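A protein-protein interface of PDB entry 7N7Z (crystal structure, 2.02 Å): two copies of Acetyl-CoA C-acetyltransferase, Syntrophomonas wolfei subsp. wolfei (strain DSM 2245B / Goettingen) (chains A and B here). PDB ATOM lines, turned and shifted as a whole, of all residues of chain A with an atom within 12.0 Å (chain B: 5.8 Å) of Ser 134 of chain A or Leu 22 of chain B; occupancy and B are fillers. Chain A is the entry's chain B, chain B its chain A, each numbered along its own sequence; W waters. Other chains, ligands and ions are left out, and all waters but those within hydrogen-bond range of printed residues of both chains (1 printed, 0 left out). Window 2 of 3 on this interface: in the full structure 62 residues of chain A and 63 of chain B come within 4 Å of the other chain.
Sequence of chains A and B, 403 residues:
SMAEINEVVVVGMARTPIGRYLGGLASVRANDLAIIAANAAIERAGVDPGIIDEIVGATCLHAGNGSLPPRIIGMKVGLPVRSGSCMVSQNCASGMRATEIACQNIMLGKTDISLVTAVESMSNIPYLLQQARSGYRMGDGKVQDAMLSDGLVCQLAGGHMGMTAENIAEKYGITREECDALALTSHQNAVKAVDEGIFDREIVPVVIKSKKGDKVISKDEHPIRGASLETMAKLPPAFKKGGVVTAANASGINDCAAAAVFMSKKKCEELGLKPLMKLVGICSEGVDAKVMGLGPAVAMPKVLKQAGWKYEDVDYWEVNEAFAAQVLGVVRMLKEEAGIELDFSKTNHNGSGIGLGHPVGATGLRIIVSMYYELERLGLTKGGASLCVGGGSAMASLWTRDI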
ATOM      1  N   LEU A 128      25.734   3.951 -24.472  1.00  0.00           N
ATOM      2  CA  LEU A 128      25.797   4.513 -23.131  1.00  0.00           C
ATOM      3  C   LEU A 128      26.291   5.954 -23.156  1.00  0.00           C
ATOM      4  O   LEU A 128      27.157   6.311 -23.961  1.00  0.00           O
ATOM      5  CB  LEU A 128      26.724   3.693 -22.228  1.00  0.00           C
ATOM      6  CG  LEU A 128      26.654   2.170 -22.313  1.00  0.00           C
ATOM      7  CD1 LEU A 128      27.850   1.561 -21.598  1.00  0.00           C
ATOM      8  CD2 LEU A 128      25.352   1.653 -21.728  1.00  0.00           C
ATOM      9  N   LEU A 129      25.740   6.769 -22.260  1.00  0.00           N
ATOM     10  CA  LEU A 129      26.250   8.106 -21.958  1.00  0.00           C
ATOM     11  C   LEU A 129      26.734   8.067 -20.510  1.00  0.00           C
ATOM     12  O   LEU A 129      25.935   8.182 -19.575  1.00  0.00           O
ATOM     13  CB  LEU A 129      25.181   9.171 -22.169  1.00  0.00           C
ATOM     14  CG  LEU A 129      24.686   9.357 -23.605  1.00  0.00           C
ATOM     15  CD1 LEU A 129      23.557  10.377 -23.647  1.00  0.00           C
ATOM     16  CD2 LEU A 129      25.825   9.779 -24.521  1.00  0.00           C
ATOM     17  N   GLN A 130      28.045   7.899 -20.329  1.00  0.00           N
ATOM     18  CA  GLN A 130      28.583   7.641 -18.998  1.00  0.00           C
ATOM     19  C   GLN A 130      28.484   8.871 -18.101  1.00  0.00           C
ATOM     20  O   GLN A 130      28.201   8.748 -16.903  1.00  0.00           O
ATOM     21  CB  GLN A 130      30.032   7.164 -19.107  1.00  0.00           C
ATOM     22  CG  GLN A 130      30.610   6.594 -17.817  1.00  0.00           C
ATOM     23  CD  GLN A 130      29.875   5.355 -17.337  1.00  0.00           C
ATOM     24  OE1 GLN A 130      30.176   4.237 -17.758  1.00  0.00           O
ATOM     25  NE2 GLN A 130      28.911   5.547 -16.442  1.00  0.00           N
ATOM     26  N   GLN A 131      28.703  10.061 -18.655  1.00  0.00           N
ATOM     27  CA  GLN A 131      28.730  11.289 -17.873  1.00  0.00           C
ATOM     28  C   GLN A 131      27.415  12.057 -17.925  1.00  0.00           C
ATOM     29  O   GLN A 131      27.372  13.219 -17.509  1.00  0.00           O
ATOM     30  CB  GLN A 131      29.870  12.188 -18.355  1.00  0.00           C
ATOM     31  CG  GLN A 131      31.137  11.435 -18.728  1.00  0.00           C
ATOM     32  CD  GLN A 131      32.391  12.212 -18.393  1.00  0.00           C
ATOM     33  OE1 GLN A 131      32.899  12.977 -19.214  1.00  0.00           O
ATOM     34  NE2 GLN A 131      32.898  12.021 -17.179  1.00  0.00           N
ATOM     35  N   ALA A 132      26.340  11.436 -18.413  1.00  0.00           N
ATOM     36  CA  ALA A 132      25.076  12.152 -18.543  1.00  0.00           C
ATOM     37  C   ALA A 132      24.461  12.474 -17.187  1.00  0.00           C
ATOM     38  O   ALA A 132      23.772  13.490 -17.048  1.00  0.00           O
ATOM     39  CB  ALA A 132      24.093  11.337 -19.382  1.00  0.00           C
ATOM     40  N   ARG A 133      24.690  11.628 -16.182  1.00  0.00           N
ATOM     41  CA  ARG A 133      24.076  11.850 -14.875  1.00  0.00           C
ATOM     42  C   ARG A 133      24.624  13.114 -14.222  1.00  0.00           C
ATOM     43  O   ARG A 133      23.877  14.059 -13.944  1.00  0.00           O
ATOM     44  CB  ARG A 133      24.305  10.633 -13.976  1.00  0.00           C
ATOM     45  CG  ARG A 133      23.435  10.615 -12.727  1.00  0.00           C
ATOM     46  CD  ARG A 133      23.521   9.275 -12.006  1.00  0.00           C
ATOM     47  NE  ARG A 133      23.126   8.169 -12.869  1.00  0.00           N
ATOM     48  CZ  ARG A 133      21.870   7.855 -13.160  1.00  0.00           C
ATOM     49  NH1 ARG A 133      20.853   8.529 -12.645  1.00  0.00           N
ATOM     50  NH2 ARG A 133      21.629   6.845 -13.991  1.00  0.00           N
ATOM     51  N   SER A 134      25.932  13.148 -13.973  1.00  0.00           N
ATOM     52  CA  SER A 134      26.552  14.301 -13.335  1.00  0.00           C
ATOM     53  C   SER A 134      26.926  15.395 -14.322  1.00  0.00           C
ATOM     54  O   SER A 134      27.180  16.530 -13.899  1.00  0.00           O
ATOM     55  CB  SER A 134      27.801  13.866 -12.565  1.00  0.00           C
ATOM     56  OG  SER A 134      27.442  13.171 -11.386  1.00  0.00           O
ATOM     57  N   GLY A 135      26.969  15.088 -15.608  1.00  0.00           N
ATOM     58  CA  GLY A 135      27.251  16.082 -16.622  1.00  0.00           C
ATOM     59  C   GLY A 135      28.677  15.997 -17.134  1.00  0.00           C
ATOM     60  O   GLY A 135      29.611  15.634 -16.410  1.00  0.00           O
ATOM     61  N   TYR A 136      28.848  16.331 -18.412  1.00  0.00           N
ATOM     62  CA  TYR A 136      30.176  16.429 -19.001  1.00  0.00           C
ATOM     63  C   TYR A 136      30.878  17.729 -18.633  1.00  0.00           C
ATOM     64  O   TYR A 136      32.075  17.868 -18.907  1.00  0.00           O
ATOM     65  CB  TYR A 136      30.083  16.299 -20.525  1.00  0.00           C
ATOM     66  CG  TYR A 136      29.573  14.954 -20.993  1.00  0.00           C
ATOM     67  CD1 TYR A 136      28.222  14.639 -20.922  1.00  0.00           C
ATOM     68  CD2 TYR A 136      30.441  14.000 -21.506  1.00  0.00           C
ATOM     69  CE1 TYR A 136      27.750  13.411 -21.347  1.00  0.00           C
ATOM     70  CE2 TYR A 136      29.978  12.769 -21.933  1.00  0.00           C
ATOM     71  CZ  TYR A 136      28.632  12.479 -21.851  1.00  0.00           C
ATOM     72  OH  TYR A 136      28.165  11.254 -22.275  1.00  0.00           O
ATOM     73  N   ARG A 137      30.164  18.676 -18.024  1.00  0.00           N
ATOM     74  CA  ARG A 137      30.747  19.920 -17.533  1.00  0.00           C
ATOM     75  C   ARG A 137      31.341  20.751 -18.666  1.00  0.00           C
ATOM     76  O   ARG A 137      30.885  21.871 -18.922  1.00  0.00           O
ATOM     77  CB  ARG A 137      31.814  19.630 -16.473  1.00  0.00           C
ATOM     78  CG  ARG A 137      31.484  18.468 -15.531  1.00  0.00           C
ATOM     79  CD  ARG A 137      30.104  18.603 -14.894  1.00  0.00           C
ATOM     80  NE  ARG A 137      29.954  19.835 -14.129  1.00  0.00           N
ATOM     81  CZ  ARG A 137      28.854  20.183 -13.477  1.00  0.00           C
ATOM     82  NH1 ARG A 137      27.776  19.415 -13.476  1.00  0.00           N
ATOM     83  NH2 ARG A 137      28.832  21.331 -12.806  1.00  0.00           N
ATOM     84  N   MET A 138      32.365  20.227 -19.336  1.00  0.00           N
ATOM     85  CA  MET A 138      32.972  20.915 -20.467  1.00  0.00           C
ATOM     86  C   MET A 138      33.809  19.914 -21.248  1.00  0.00           C
ATOM     87  O   MET A 138      34.338  18.953 -20.683  1.00  0.00           O
ATOM     88  CB  MET A 138      33.834  22.100 -20.015  1.00  0.00           C
ATOM     89  CG  MET A 138      34.389  22.932 -21.165  1.00  0.00           C
ATOM     90  SD  MET A 138      34.974  24.561 -20.660  1.00  0.00           S
ATOM     91  CE  MET A 138      36.724  24.239 -20.448  1.00  0.00           C
ATOM     92  N   GLY A 139      33.911  20.143 -22.551  1.00  0.00           N
ATOM     93  CA  GLY A 139      34.697  19.291 -23.417  1.00  0.00           C
ATOM     94  C   GLY A 139      33.922  18.078 -23.903  1.00  0.00           C
ATOM     95  O   GLY A 139      32.876  17.709 -23.371  1.00  0.00           O
ATOM     96  N   GLY A 141      32.995  14.134 -24.881  1.00  0.00           N
ATOM     97  CA  GLY A 141      33.061  12.828 -24.260  1.00  0.00           C
ATOM     98  C   GLY A 141      32.920  11.746 -25.309  1.00  0.00           C
ATOM     99  O   GLY A 141      33.126  12.003 -26.499  1.00  0.00           O
ATOM    100  N   ARG B  20      26.190   8.751  -0.291  1.00  0.00           N
ATOM    101  CA  ARG B  20      24.950   9.347  -0.760  1.00  0.00           C
ATOM    102  C   ARG B  20      24.939   9.427  -2.280  1.00  0.00           C
ATOM    103  O   ARG B  20      25.985   9.554  -2.924  1.00  0.00           O
ATOM    104  CB  ARG B  20      24.769  10.747  -0.173  1.00  0.00           C
ATOM    105  CG  ARG B  20      23.424  10.970   0.502  1.00  0.00           C
ATOM    106  CD  ARG B  20      23.116  12.453   0.662  1.00  0.00           C
ATOM    107  NE  ARG B  20      23.193  12.883   2.053  1.00  0.00           N
ATOM    108  CZ  ARG B  20      22.237  12.690   2.952  1.00  0.00           C
ATOM    109  NH1 ARG B  20      21.113  12.062   2.644  1.00  0.00           N
ATOM    110  NH2 ARG B  20      22.413  13.139   4.191  1.00  0.00           N
ATOM    111  N   TYR B  21      23.740   9.352  -2.851  1.00  0.00           N
ATOM    112  CA  TYR B  21      23.577   9.499  -4.292  1.00  0.00           C
ATOM    113  C   TYR B  21      24.258  10.772  -4.769  1.00  0.00           C
ATOM    114  O   TYR B  21      23.926  11.872  -4.318  1.00  0.00           O
ATOM    115  CB  TYR B  21      22.090   9.522  -4.645  1.00  0.00           C
ATOM    116  CG  TYR B  21      21.798   9.702  -6.118  1.00  0.00           C
ATOM    117  CD1 TYR B  21      22.042   8.679  -7.024  1.00  0.00           C
ATOM    118  CD2 TYR B  21      21.264  10.888  -6.599  1.00  0.00           C
ATOM    119  CE1 TYR B  21      21.767   8.835  -8.367  1.00  0.00           C
ATOM    120  CE2 TYR B  21      20.988  11.055  -7.941  1.00  0.00           C
ATOM    121  CZ  TYR B  21      21.242  10.024  -8.821  1.00  0.00           C
ATOM    122  OH  TYR B  21      20.966  10.185 -10.160  1.00  0.00           O
ATOM    123  N   LEU B  22      25.221  10.618  -5.678  1.00  0.00           N
ATOM    124  CA  LEU B  22      26.013  11.742  -6.175  1.00  0.00           C
ATOM    125  C   LEU B  22      26.758  12.438  -5.040  1.00  0.00           C
ATOM    126  O   LEU B  22      26.976  13.652  -5.079  1.00  0.00           O
ATOM    127  CB  LEU B  22      25.138  12.748  -6.927  1.00  0.00           C
ATOM    128  CG  LEU B  22      24.388  12.203  -8.143  1.00  0.00           C
ATOM    129  CD1 LEU B  22      23.443  13.253  -8.701  1.00  0.00           C
ATOM    130  CD2 LEU B  22      25.367  11.737  -9.209  1.00  0.00           C
ATOM    131  N   GLY B  23      27.158  11.672  -4.027  1.00  0.00           N
ATOM    132  CA  GLY B  23      27.777  12.238  -2.846  1.00  0.00           C
ATOM    133  C   GLY B  23      29.273  12.013  -2.749  1.00  0.00           C
ATOM    134  O   GLY B  23      30.010  12.245  -3.713  1.00  0.00           O
ATOM    135  N   GLY B  24      29.729  11.554  -1.582  1.00  0.00           N
ATOM    136  CA  GLY B  24      31.156  11.467  -1.329  1.00  0.00           C
ATOM    137  C   GLY B  24      31.871  10.431  -2.174  1.00  0.00           C
ATOM    138  O   GLY B  24      33.070  10.565  -2.437  1.00  0.00           O
ATOM    139  N   ALA B  26      30.734   9.497  -5.295  1.00  0.00           N
ATOM    140  CA  ALA B  26      30.279   9.600  -6.677  1.00  0.00           C
ATOM    141  C   ALA B  26      31.430   9.488  -7.669  1.00  0.00           C
ATOM    142  O   ALA B  26      31.216   9.095  -8.822  1.00  0.00           O
ATOM    143  CB  ALA B  26      29.536  10.920  -6.883  1.00  0.00           C
ATOM    144  N   MET B 122      25.451   3.709  -7.801  1.00  0.00           N
ATOM    145  CA  MET B 122      24.305   4.324  -8.457  1.00  0.00           C
ATOM    146  C   MET B 122      24.611   5.736  -8.932  1.00  0.00           C
ATOM    147  O   MET B 122      23.957   6.218  -9.863  1.00  0.00           O
ATOM    148  CB  MET B 122      23.107   4.309  -7.505  1.00  0.00           C
ATOM    149  CG  MET B 122      22.776   2.904  -6.998  1.00  0.00           C
ATOM    150  SD  MET B 122      21.275   2.795  -6.004  1.00  0.00           S
ATOM    151  CE  MET B 122      20.039   2.621  -7.287  1.00  0.00           C
ATOM    152  N   SER B 123      25.601   6.401  -8.330  1.00  0.00           N
ATOM    153  CA  SER B 123      26.036   7.704  -8.820  1.00  0.00           C
ATOM    154  C   SER B 123      26.672   7.617 -10.201  1.00  0.00           C
ATOM    155  O   SER B 123      26.731   8.630 -10.907  1.00  0.00           O
ATOM    156  CB  SER B 123      27.032   8.331  -7.843  1.00  0.00           C
ATOM    157  OG  SER B 123      26.497   8.423  -6.534  1.00  0.00           O
ATOM    158  N   ASN B 124      27.151   6.437 -10.600  1.00  0.00           N
ATOM    159  CA  ASN B 124      27.864   6.264 -11.859  1.00  0.00           C
ATOM    160  C   ASN B 124      27.116   5.367 -12.841  1.00  0.00           C
ATOM    161  O   ASN B 124      27.712   4.884 -13.811  1.00  0.00           O
ATOM    162  CB  ASN B 124      29.264   5.707 -11.594  1.00  0.00           C
ATOM    163  CG  ASN B 124      30.193   6.739 -10.988  1.00  0.00           C
ATOM    164  OD1 ASN B 124      30.566   7.713 -11.641  1.00  0.00           O
ATOM    165  ND2 ASN B 124      30.569   6.532  -9.732  1.00  0.00           N
ATOM    166  N   ASP B 255      25.656   4.472  -2.847  1.00  0.00           N
ATOM    167  CA  ASP B 255      26.805   3.764  -3.389  1.00  0.00           C
ATOM    168  C   ASP B 255      27.493   3.001  -2.266  1.00  0.00           C
ATOM    169  O   ASP B 255      27.595   3.499  -1.138  1.00  0.00           O
ATOM    170  CB  ASP B 255      27.799   4.736  -4.040  1.00  0.00           C
ATOM    171  CG  ASP B 255      27.122   5.754  -4.938  1.00  0.00           C
ATOM    172  OD1 ASP B 255      26.197   5.369  -5.684  1.00  0.00           O
ATOM    173  OD2 ASP B 255      27.517   6.940  -4.899  1.00  0.00           O
HETATM  174  O   HOH W   1      29.721   7.952 -14.366  1.00  0.00           O
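Met 122 of chain B touches Arg 133 of chain A.
Ser 123 of chain B touches Arg 133 of chain A (O to CD, 3.5 Å).
CD2 of Leu 22 of chain B touches OG of Ser 134 of chain A, at 3.3 Å.
Printed residues of chain B that touch a printed residue of chain A: Tyr 21, Leu 22, Met 122, Ser 123 and Asn 124.
Hydrophobic or aromatic side chains of chain B within 4 Å of the printed part of chain A: Tyr 21 and Leu 22.
Along chain B the printed residues that touch a printed residue of chain A span positions 21 to 124.
Among the printed residues, 5 pairs touch across the chains.
Among the printed residues, no Asp or Glu carboxylate lies within 4 Å of a Lys or Arg side-chain nitrogen of the other chain.
Printed residues of chain B within 4 Å of Gln 130 of chain A: Asn 124 (3.0 Å).
Ala 132 of chain A touches none of the printed residues of chain B.
Of chain B, only Leu 22 (3.3 Å) comes within 4 Å of Ser 134 of chain A.
Of chain A, only Arg 133 comes within 4 Å of Tyr 21 of chain B.
Of chain A, only Ser 134 (3.3 Å) comes within 4 Å of Leu 22 of chain B.
No residue of chain A comes within 4 Å of Gly 23 of chain B.
No residue of chain A comes within 4 Å of Ala 26 of chain B.
Printed residues of chain A within 4 Å of Met 122 of chain B: Arg 133.
The nearest residue of chain A that does not touch Leu 22 of chain B is Arg 133 of chain A (4.2 Å).
No position is printed for both chains.
Water W1 bridges the side-chain amide oxygen (OD1) of Asn 124 of chain B and the backbone carbonyl oxygen (O) of Gln 130 of chain A.
OG of Ser 123 of chain B lies within hydrogen-bond range of OD2 of Asp 255 of chain B (2.4 Å).
OG of Ser 123 of chain B lies within hydrogen-bond range of N of Leu 22 of chain B, 2.7 Å away.
O of Ser 134 of chain A is in hydrogen-bond range of NH1 of Arg 137 of chain A, 3.0 Å away.
The backbone NH (N) of Met 122 of chain B is in hydrogen-bond range of the side-chain carboxylate (OD1) of Asp 255 of chain B, at 2.8 Å.
The backbone carbonyl oxygen (O) of Ala 26 of chain B sits at hydrogen-bond distance from the side-chain amide nitrogen (ND2) of Asn 124 of chain B, at 2.8 Å.
O of Asn 124 of chain B sits at hydrogen-bond distance from NE2 of Gln 130 of chain A (3.0 Å).
The side-chain hydroxyl (OH) of Tyr 21 of chain B sits at hydrogen-bond distance from the guanidinium group (NH1) of Arg 133 of chain A (3.0 Å).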
